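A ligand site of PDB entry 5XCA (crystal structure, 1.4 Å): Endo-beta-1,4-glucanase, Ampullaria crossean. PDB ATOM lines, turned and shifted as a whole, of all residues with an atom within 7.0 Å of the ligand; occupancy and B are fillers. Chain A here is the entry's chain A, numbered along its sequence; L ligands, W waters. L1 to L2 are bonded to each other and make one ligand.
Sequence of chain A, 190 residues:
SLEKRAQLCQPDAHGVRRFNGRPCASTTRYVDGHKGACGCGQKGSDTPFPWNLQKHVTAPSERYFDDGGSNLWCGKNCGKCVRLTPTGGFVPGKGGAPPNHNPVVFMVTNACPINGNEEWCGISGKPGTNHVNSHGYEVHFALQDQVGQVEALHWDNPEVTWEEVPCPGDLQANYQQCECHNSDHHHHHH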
ATOM      1  N   TYR A  30     -32.184  16.261  -5.160  1.00  0.00           N
ATOM      2  CA  TYR A  30     -30.823  15.790  -5.293  1.00  0.00           C
ATOM      3  C   TYR A  30     -29.860  16.948  -5.148  1.00  0.00           C
ATOM      4  O   TYR A  30     -30.219  18.106  -5.396  1.00  0.00           O
ATOM      5  CB  TYR A  30     -30.589  15.037  -6.607  1.00  0.00           C
ATOM      6  CG  TYR A  30     -30.279  15.862  -7.831  1.00  0.00           C
ATOM      7  CD1 TYR A  30     -31.289  16.532  -8.516  1.00  0.00           C
ATOM      8  CD2 TYR A  30     -28.982  15.940  -8.314  1.00  0.00           C
ATOM      9  CE1 TYR A  30     -31.021  17.244  -9.664  1.00  0.00           C
ATOM     10  CE2 TYR A  30     -28.697  16.678  -9.468  1.00  0.00           C
ATOM     11  CZ  TYR A  30     -29.699  17.344 -10.118  1.00  0.00           C
ATOM     12  OH  TYR A  30     -29.422  18.027 -11.285  1.00  0.00           O
ATOM     13  N   VAL A  31     -28.622  16.620  -4.772  1.00  0.00           N
ATOM     14  CA  VAL A  31     -27.510  17.554  -4.811  1.00  0.00           C
ATOM     15  C   VAL A  31     -26.307  16.766  -5.310  1.00  0.00           C
ATOM     16  O   VAL A  31     -26.107  15.617  -4.912  1.00  0.00           O
ATOM     17  CB  VAL A  31     -27.210  18.160  -3.422  1.00  0.00           C
ATOM     18  CG1 VAL A  31     -28.348  19.025  -2.939  1.00  0.00           C
ATOM     19  CG2 VAL A  31     -26.913  17.076  -2.404  1.00  0.00           C
ATOM     20  N   ASP A  32     -25.522  17.347  -6.187  1.00  0.00           N
ATOM     21  CA  ASP A  32     -24.274  16.669  -6.524  1.00  0.00           C
ATOM     22  C   ASP A  32     -23.189  17.605  -7.010  1.00  0.00           C
ATOM     23  O   ASP A  32     -22.033  17.166  -7.116  1.00  0.00           O
ATOM     24  CB  ASP A  32     -24.494  15.477  -7.470  1.00  0.00           C
ATOM     25  CG  ASP A  32     -24.964  15.880  -8.867  1.00  0.00           C
ATOM     26  OD1 ASP A  32     -24.790  17.046  -9.290  1.00  0.00           O
ATOM     27  OD2 ASP A  32     -25.485  14.960  -9.578  1.00  0.00           O
ATOM     28  N   GLY A  33     -23.511  18.869  -7.311  1.00  0.00           N
ATOM     29  CA  GLY A  33     -22.503  19.853  -7.657  1.00  0.00           C
ATOM     30  C   GLY A  33     -21.940  19.730  -9.063  1.00  0.00           C
ATOM     31  O   GLY A  33     -21.086  20.552  -9.432  1.00  0.00           O
ATOM     32  N   HIS A  34     -22.379  18.730  -9.849  1.00  0.00           N
ATOM     33  CA  HIS A  34     -21.848  18.588 -11.212  1.00  0.00           C
ATOM     34  C   HIS A  34     -22.460  19.642 -12.136  1.00  0.00           C
ATOM     35  O   HIS A  34     -23.551  20.163 -11.898  1.00  0.00           O
ATOM     36  CB  HIS A  34     -22.143  17.180 -11.759  1.00  0.00           C
ATOM     37  CG  HIS A  34     -21.391  16.100 -11.037  1.00  0.00           C
ATOM     38  ND1 HIS A  34     -20.013  16.006 -11.054  1.00  0.00           N
ATOM     39  CD2 HIS A  34     -21.814  15.103 -10.225  1.00  0.00           C
ATOM     40  CE1 HIS A  34     -19.624  14.993 -10.304  1.00  0.00           C
ATOM     41  NE2 HIS A  34     -20.706  14.421  -9.786  1.00  0.00           N
ATOM     42  N   LYS A  35     -21.732  19.930 -13.230  1.00  0.00           N
ATOM     43  CA  LYS A  35     -22.305  20.776 -14.288  1.00  0.00           C
ATOM     44  C   LYS A  35     -23.600  20.173 -14.813  1.00  0.00           C
ATOM     45  O   LYS A  35     -24.619  20.870 -14.937  1.00  0.00           O
ATOM     46  CB  LYS A  35     -21.281  20.904 -15.421  1.00  0.00           C
ATOM     47  CG  LYS A  35     -21.839  21.610 -16.663  1.00  0.00           C
ATOM     48  CD  LYS A  35     -20.733  22.114 -17.572  1.00  0.00           C
ATOM     49  CE  LYS A  35     -20.013  20.968 -18.267  1.00  0.00           C
ATOM     50  NZ  LYS A  35     -19.010  21.499 -19.195  1.00  0.00           N
ATOM     51  N   GLY A  36     -23.589  18.900 -15.126  1.00  0.00           N
ATOM     52  CA  GLY A  36     -24.811  18.226 -15.526  1.00  0.00           C
ATOM     53  C   GLY A  36     -24.859  17.931 -17.024  1.00  0.00           C
ATOM     54  O   GLY A  36     -24.042  18.419 -17.829  1.00  0.00           O
ATOM     55  N   ALA A  37     -25.869  17.131 -17.393  1.00  0.00           N
ATOM     56  CA  ALA A  37     -25.908  16.473 -18.694  1.00  0.00           C
ATOM     57  C   ALA A  37     -26.373  17.368 -19.815  1.00  0.00           C
ATOM     58  O   ALA A  37     -26.292  16.948 -20.975  1.00  0.00           O
ATOM     59  CB  ALA A  37     -26.804  15.235 -18.614  1.00  0.00           C
ATOM     60  N   CYS A  38     -26.779  18.612 -19.519  1.00  0.00           N
ATOM     61  CA  CYS A  38     -27.150  19.563 -20.557  1.00  0.00           C
ATOM     62  C   CYS A  38     -26.039  20.599 -20.784  1.00  0.00           C
ATOM     63  O   CYS A  38     -26.229  21.576 -21.528  1.00  0.00           O
ATOM     64  CB  CYS A  38     -28.478  20.228 -20.219  1.00  0.00           C
ATOM     65  SG  CYS A  38     -29.828  19.010 -20.207  1.00  0.00           S
ATOM     66  N   GLY A  39     -24.875  20.413 -20.149  1.00  0.00           N
ATOM     67  CA  GLY A  39     -23.800  21.367 -20.363  1.00  0.00           C
ATOM     68  C   GLY A  39     -24.017  22.765 -19.819  1.00  0.00           C
ATOM     69  O   GLY A  39     -23.465  23.738 -20.373  1.00  0.00           O
ATOM     70  N   SER A  45     -15.277  22.025 -18.393  1.00  0.00           N
ATOM     71  CA  SER A  45     -15.084  21.914 -16.958  1.00  0.00           C
ATOM     72  C   SER A  45     -16.368  21.417 -16.310  1.00  0.00           C
ATOM     73  O   SER A  45     -17.470  21.776 -16.749  1.00  0.00           O
ATOM     74  CB  SER A  45     -14.754  23.273 -16.344  1.00  0.00           C
ATOM     75  OG  SER A  45     -14.907  23.185 -14.937  1.00  0.00           O
ATOM     76  N   ASP A  46     -16.238  20.617 -15.263  1.00  0.00           N
ATOM     77  CA  ASP A  46     -17.405  20.151 -14.509  1.00  0.00           C
ATOM     78  C   ASP A  46     -17.879  21.187 -13.481  1.00  0.00           C
ATOM     79  O   ASP A  46     -18.056  20.874 -12.299  1.00  0.00           O
ATOM     80  CB  ASP A  46     -17.113  18.806 -13.817  1.00  0.00           C
ATOM     81  CG  ASP A  46     -18.380  18.148 -13.259  1.00  0.00           C
ATOM     82  OD1 ASP A  46     -19.458  18.314 -13.861  1.00  0.00           O
ATOM     83  OD2 ASP A  46     -18.294  17.520 -12.164  1.00  0.00           O
ATOM     84  N   THR A  47     -18.074  22.436 -13.915  1.00  0.00           N
ATOM     85  CA  THR A  47     -18.476  23.523 -13.022  1.00  0.00           C
ATOM     86  C   THR A  47     -19.809  24.060 -13.523  1.00  0.00           C
ATOM     87  O   THR A  47     -19.855  24.689 -14.601  1.00  0.00           O
ATOM     88  CB  THR A  47     -17.421  24.627 -13.025  1.00  0.00           C
ATOM     89  OG1 THR A  47     -16.167  24.081 -12.599  1.00  0.00           O
ATOM     90  CG2 THR A  47     -17.846  25.765 -12.079  1.00  0.00           C
ATOM     91  N   ALA A  59     -33.297  17.056 -12.998  1.00  0.00           N
ATOM     92  CA  ALA A  59     -32.737  15.911 -13.723  1.00  0.00           C
ATOM     93  C   ALA A  59     -33.852  14.874 -13.874  1.00  0.00           C
ATOM     94  O   ALA A  59     -34.142  14.114 -12.917  1.00  0.00           O
ATOM     95  CB  ALA A  59     -31.555  15.313 -12.946  1.00  0.00           C
ATOM     96  N   PHE A  65     -35.595  12.285 -20.342  1.00  0.00           N
ATOM     97  CA  PHE A  65     -34.464  13.161 -20.637  1.00  0.00           C
ATOM     98  C   PHE A  65     -34.054  13.105 -22.096  1.00  0.00           C
ATOM     99  O   PHE A  65     -33.862  14.157 -22.712  1.00  0.00           O
ATOM    100  CB  PHE A  65     -33.288  12.792 -19.740  1.00  0.00           C
ATOM    101  CG  PHE A  65     -32.042  13.539 -20.064  1.00  0.00           C
ATOM    102  CD1 PHE A  65     -31.871  14.807 -19.575  1.00  0.00           C
ATOM    103  CD2 PHE A  65     -31.005  12.960 -20.842  1.00  0.00           C
ATOM    104  CE1 PHE A  65     -30.746  15.519 -19.844  1.00  0.00           C
ATOM    105  CE2 PHE A  65     -29.855  13.688 -21.123  1.00  0.00           C
ATOM    106  CZ  PHE A  65     -29.746  14.955 -20.612  1.00  0.00           C
ATOM    107  N   ASN A  71     -28.867   8.683 -24.493  1.00  0.00           N
ATOM    108  CA  ASN A  71     -27.823   9.713 -24.428  1.00  0.00           C
ATOM    109  C   ASN A  71     -27.868  10.458 -23.120  1.00  0.00           C
ATOM    110  O   ASN A  71     -28.929  10.923 -22.683  1.00  0.00           O
ATOM    111  CB  ASN A  71     -27.990  10.685 -25.577  1.00  0.00           C
ATOM    112  CG  ASN A  71     -27.533  10.075 -26.859  1.00  0.00           C
ATOM    113  OD1 ASN A  71     -26.443   9.520 -26.913  1.00  0.00           O
ATOM    114  ND2 ASN A  71     -28.382  10.126 -27.873  1.00  0.00           N
ATOM    115  N   LEU A  72     -26.719  10.560 -22.484  1.00  0.00           N
ATOM    116  CA  LEU A  72     -26.618  11.278 -21.226  1.00  0.00           C
ATOM    117  C   LEU A  72     -25.819  12.558 -21.393  1.00  0.00           C
ATOM    118  O   LEU A  72     -25.392  13.143 -20.394  1.00  0.00           O
ATOM    119  CB  LEU A  72     -25.977  10.399 -20.154  1.00  0.00           C
ATOM    120  CG  LEU A  72     -26.814   9.199 -19.743  1.00  0.00           C
ATOM    121  CD1 LEU A  72     -26.073   8.392 -18.755  1.00  0.00           C
ATOM    122  CD2 LEU A  72     -28.212   9.622 -19.255  1.00  0.00           C
ATOM    123  N   TRP A  73     -25.647  13.012 -22.626  1.00  0.00           N
ATOM    124  CA  TRP A  73     -25.072  14.322 -22.932  1.00  0.00           C
ATOM    125  C   TRP A  73     -25.957  14.963 -23.993  1.00  0.00           C
ATOM    126  O   TRP A  73     -26.152  14.384 -25.071  1.00  0.00           O
ATOM    127  CB  TRP A  73     -23.647  14.178 -23.451  1.00  0.00           C
ATOM    128  CG  TRP A  73     -22.998  15.477 -23.879  1.00  0.00           C
ATOM    129  CD1 TRP A  73     -22.641  15.842 -25.154  1.00  0.00           C
ATOM    130  CD2 TRP A  73     -22.675  16.578 -23.032  1.00  0.00           C
ATOM    131  NE1 TRP A  73     -22.117  17.103 -25.138  1.00  0.00           N
ATOM    132  CE2 TRP A  73     -22.112  17.579 -23.853  1.00  0.00           C
ATOM    133  CE3 TRP A  73     -22.807  16.823 -21.655  1.00  0.00           C
ATOM    134  CZ2 TRP A  73     -21.693  18.782 -23.360  1.00  0.00           C
ATOM    135  CZ3 TRP A  73     -22.339  18.030 -21.155  1.00  0.00           C
ATOM    136  CH2 TRP A  73     -21.792  18.998 -22.010  1.00  0.00           C
ATOM    137  N   CYS A  74     -26.461  16.165 -23.722  1.00  0.00           N
ATOM    138  CA  CYS A  74     -27.373  16.825 -24.645  1.00  0.00           C
ATOM    139  C   CYS A  74     -28.543  15.915 -25.035  1.00  0.00           C
ATOM    140  O   CYS A  74     -28.809  15.661 -26.222  1.00  0.00           O
ATOM    141  CB  CYS A  74     -26.666  17.352 -25.904  1.00  0.00           C
ATOM    142  SG  CYS A  74     -25.268  18.488 -25.522  1.00  0.00           S
ATOM    143  N   ASN A 110     -30.294  18.405 -16.544  1.00  0.00           N
ATOM    144  CA  ASN A 110     -29.443  17.280 -16.187  1.00  0.00           C
ATOM    145  C   ASN A 110     -30.287  16.037 -16.366  1.00  0.00           C
ATOM    146  O   ASN A 110     -31.489  16.113 -16.655  1.00  0.00           O
ATOM    147  CB  ASN A 110     -28.933  17.465 -14.748  1.00  0.00           C
ATOM    148  CG  ASN A 110     -27.812  16.522 -14.364  1.00  0.00           C
ATOM    149  OD1 ASN A 110     -27.196  15.859 -15.221  1.00  0.00           O
ATOM    150  ND2 ASN A 110     -27.493  16.493 -13.066  1.00  0.00           N
ATOM    151  N   ALA A 111     -29.663  14.870 -16.143  1.00  0.00           N
ATOM    152  CA  ALA A 111     -30.310  13.579 -16.311  1.00  0.00           C
ATOM    153  C   ALA A 111     -30.211  12.723 -15.044  1.00  0.00           C
ATOM    154  O   ALA A 111     -29.207  12.777 -14.309  1.00  0.00           O
ATOM    155  CB  ALA A 111     -29.688  12.784 -17.485  1.00  0.00           C
ATOM    156  N   CYS A 112     -31.279  11.938 -14.792  1.00  0.00           N
ATOM    157  CA  CYS A 112     -31.291  10.898 -13.770  1.00  0.00           C
ATOM    158  C   CYS A 112     -31.128   9.544 -14.470  1.00  0.00           C
ATOM    159  O   CYS A 112     -32.132   8.971 -14.963  1.00  0.00           O
ATOM    160  CB  CYS A 112     -32.582  10.948 -12.998  1.00  0.00           C
ATOM    161  SG  CYS A 112     -32.681   9.752 -11.580  1.00  0.00           S
ATOM    162  N   PRO A 113     -29.924   9.003 -14.551  1.00  0.00           N
ATOM    163  CA  PRO A 113     -29.741   7.772 -15.324  1.00  0.00           C
ATOM    164  C   PRO A 113     -30.367   6.594 -14.623  1.00  0.00           C
ATOM    165  O   PRO A 113     -30.414   6.542 -13.382  1.00  0.00           O
ATOM    166  CB  PRO A 113     -28.230   7.604 -15.377  1.00  0.00           C
ATOM    167  CG  PRO A 113     -27.675   8.477 -14.373  1.00  0.00           C
ATOM    168  CD  PRO A 113     -28.659   9.534 -14.006  1.00  0.00           C
ATOM    169  N   ASN A 115     -29.019   3.720 -14.448  1.00  0.00           N
ATOM    170  CA  ASN A 115     -27.953   3.050 -13.721  1.00  0.00           C
ATOM    171  C   ASN A 115     -27.691   3.815 -12.428  1.00  0.00           C
ATOM    172  O   ASN A 115     -27.328   4.997 -12.456  1.00  0.00           O
ATOM    173  CB  ASN A 115     -26.690   3.053 -14.592  1.00  0.00           C
ATOM    174  CG  ASN A 115     -25.553   2.214 -14.006  1.00  0.00           C
ATOM    175  OD1 ASN A 115     -25.799   1.186 -13.334  1.00  0.00           O
ATOM    176  ND2 ASN A 115     -24.303   2.637 -14.245  1.00  0.00           N
ATOM    177  N   ASN A 117     -30.050   4.481 -10.207  1.00  0.00           N
ATOM    178  CA  ASN A 117     -31.276   5.104  -9.738  1.00  0.00           C
ATOM    179  C   ASN A 117     -32.471   4.245 -10.098  1.00  0.00           C
ATOM    180  O   ASN A 117     -33.433   4.712 -10.701  1.00  0.00           O
ATOM    181  CB  ASN A 117     -31.467   6.480 -10.347  1.00  0.00           C
ATOM    182  CG  ASN A 117     -30.339   7.452  -9.987  1.00  0.00           C
ATOM    183  OD1 ASN A 117     -30.351   8.033  -8.883  1.00  0.00           O
ATOM    184  ND2 ASN A 117     -29.380   7.645 -10.885  1.00  0.00           N
ATOM    185  N   GLN A 144     -33.122  19.709  -8.252  1.00  0.00           N
ATOM    186  CA  GLN A 144     -31.891  20.297  -7.701  1.00  0.00           C
ATOM    187  C   GLN A 144     -32.181  21.067  -6.425  1.00  0.00           C
ATOM    188  O   GLN A 144     -33.104  21.892  -6.385  1.00  0.00           O
ATOM    189  CB  GLN A 144     -31.346  21.237  -8.773  1.00  0.00           C
ATOM    190  CG  GLN A 144     -30.037  21.987  -8.321  1.00  0.00           C
ATOM    191  CD  GLN A 144     -28.859  21.044  -8.003  1.00  0.00           C
ATOM    192  OE1 GLN A 144     -28.500  20.851  -6.843  1.00  0.00           O
ATOM    193  NE2 GLN A 144     -28.228  20.509  -9.054  1.00  0.00           N
HETATM  194  C1  LIG L   1     -25.035  13.849 -12.794  1.00  0.00           C
HETATM  195  C2  LIG L   1     -24.526  14.285 -14.165  1.00  0.00           C
HETATM  196  C3  LIG L   1     -24.519  13.136 -15.194  1.00  0.00           C
HETATM  197  C4  LIG L   1     -25.824  12.340 -15.165  1.00  0.00           C
HETATM  198  C5  LIG L   1     -25.725  11.059 -15.999  1.00  0.00           C
HETATM  199  C6  LIG L   1     -26.367  13.119 -12.977  1.00  0.00           C
HETATM  200  O1  LIG L   1     -26.890  12.650 -11.727  1.00  0.00           O
HETATM  201  O2  LIG L   1     -25.205  14.992 -11.966  1.00  0.00           O
HETATM  202  O3  LIG L   1     -23.211  14.859 -14.005  1.00  0.00           O
HETATM  203  O4  LIG L   1     -24.439  13.638 -16.537  1.00  0.00           O
HETATM  204  O5  LIG L   1     -26.151  11.996 -13.816  1.00  0.00           O
HETATM  205  O6  LIG L   1     -24.662  10.255 -15.471  1.00  0.00           O
HETATM  206  C1  LG2 L   2     -23.118  13.778 -18.505  1.00  0.00           C
HETATM  207  C2  LG2 L   2     -21.676  13.953 -18.965  1.00  0.00           C
HETATM  208  C3  LG2 L   2     -21.252  15.370 -18.591  1.00  0.00           C
HETATM  209  C4  LG2 L   2     -21.394  15.583 -17.065  1.00  0.00           C
HETATM  210  C5  LG2 L   2     -21.036  16.996 -16.616  1.00  0.00           C
HETATM  211  C6  LG2 L   2     -23.129  13.942 -16.992  1.00  0.00           C
HETATM  212  O1  LG2 L   2     -23.581  12.455 -18.769  1.00  0.00           O
HETATM  213  O2  LG2 L   2     -21.587  13.707 -20.381  1.00  0.00           O
HETATM  214  O3  LG2 L   2     -19.917  15.530 -19.065  1.00  0.00           O
HETATM  215  O4  LG2 L   2     -22.748  15.281 -16.641  1.00  0.00           O
HETATM  216  O5  LG2 L   2     -21.386  17.097 -15.227  1.00  0.00           O
HETATM  217  O   HOH W   1     -22.192  11.219 -21.619  1.00  0.00           O
HETATM  218  O   HOH W   2     -29.450  12.522 -10.711  1.00  0.00           O
HETATM  219  O   HOH W   3     -27.425   9.911 -10.465  1.00  0.00           O
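His 34 touches the ligand. CB of Ala 37 touches O4 of LIG L1, 3.5 Å away. Trp 73 touches the ligand. CD of Pro 113 touches O5 of LIG L1 (3.5 Å). Hydrophobic or aromatic side chains within 4 Å of the ligand: His 34, Ala 37, Leu 72, Trp 73 and Pro 113. Of the 26 residues printed, 11 come within 4 Å of the ligand. Along chain A the residues within 4 Å of the ligand span positions 32 to 113.
The side-chain carboxylate (OD1) of Asp 46 lies within hydrogen-bond range of the backbone NH (N) of Lys 35. The side-chain carboxylate of Asp 32 sits at hydrogen-bond distance from the backbone NH of His 34 (3.0 Å). The backbone NH (N) of Cys 74 is in hydrogen-bond range of the backbone carbonyl oxygen (O) of Ala 37 (2.9 Å). The backbone NH (N) of Asn 110 is in hydrogen-bond range of the side-chain sulfur (SG) of Cys 38 (3.7 Å). ND1 of His 34 is in hydrogen-bond range of OD2 of Asp 46, at 2.5 Å. The side-chain amino group (NZ) of Lys 35 lies within hydrogen-bond range of the backbone carbonyl oxygen (O) of Ser 45. The backbone carbonyl oxygen of Pro 113 sits at hydrogen-bond distance from the side-chain amide nitrogen of Asn 117. OD1 of Asn 110 is in hydrogen-bond range of N of Ala 37, at 2.8 Å.
OD2 of Asp 32 lies within hydrogen-bond range of O2 of LIG L1 (2.4 Å). O5 of LG2 L2 is in hydrogen-bond range of N of Gly 36. The side-chain carboxylate (OD1) of Asp 46 is in hydrogen-bond range of an oxygen (O5) of LG2 L2 (2.7 Å). O of Ala 111 sits close to O1 of LIG L1. The backbone carbonyl oxygen (O) of Leu 72 sits at hydrogen-bond distance from an oxygen (O1) of LG2 L2, 2.5 Å away. An oxygen (O5) of LG2 L2 sits at hydrogen-bond distance from the backbone NH of Lys 35 (3.5 Å). ND2 of Asn 110 lies within hydrogen-bond range of O2 of LIG L1.
Water W3 bridges ND2 of Asn 117 (3.0 Å) and O1 of LIG L1 (3.1 Å).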
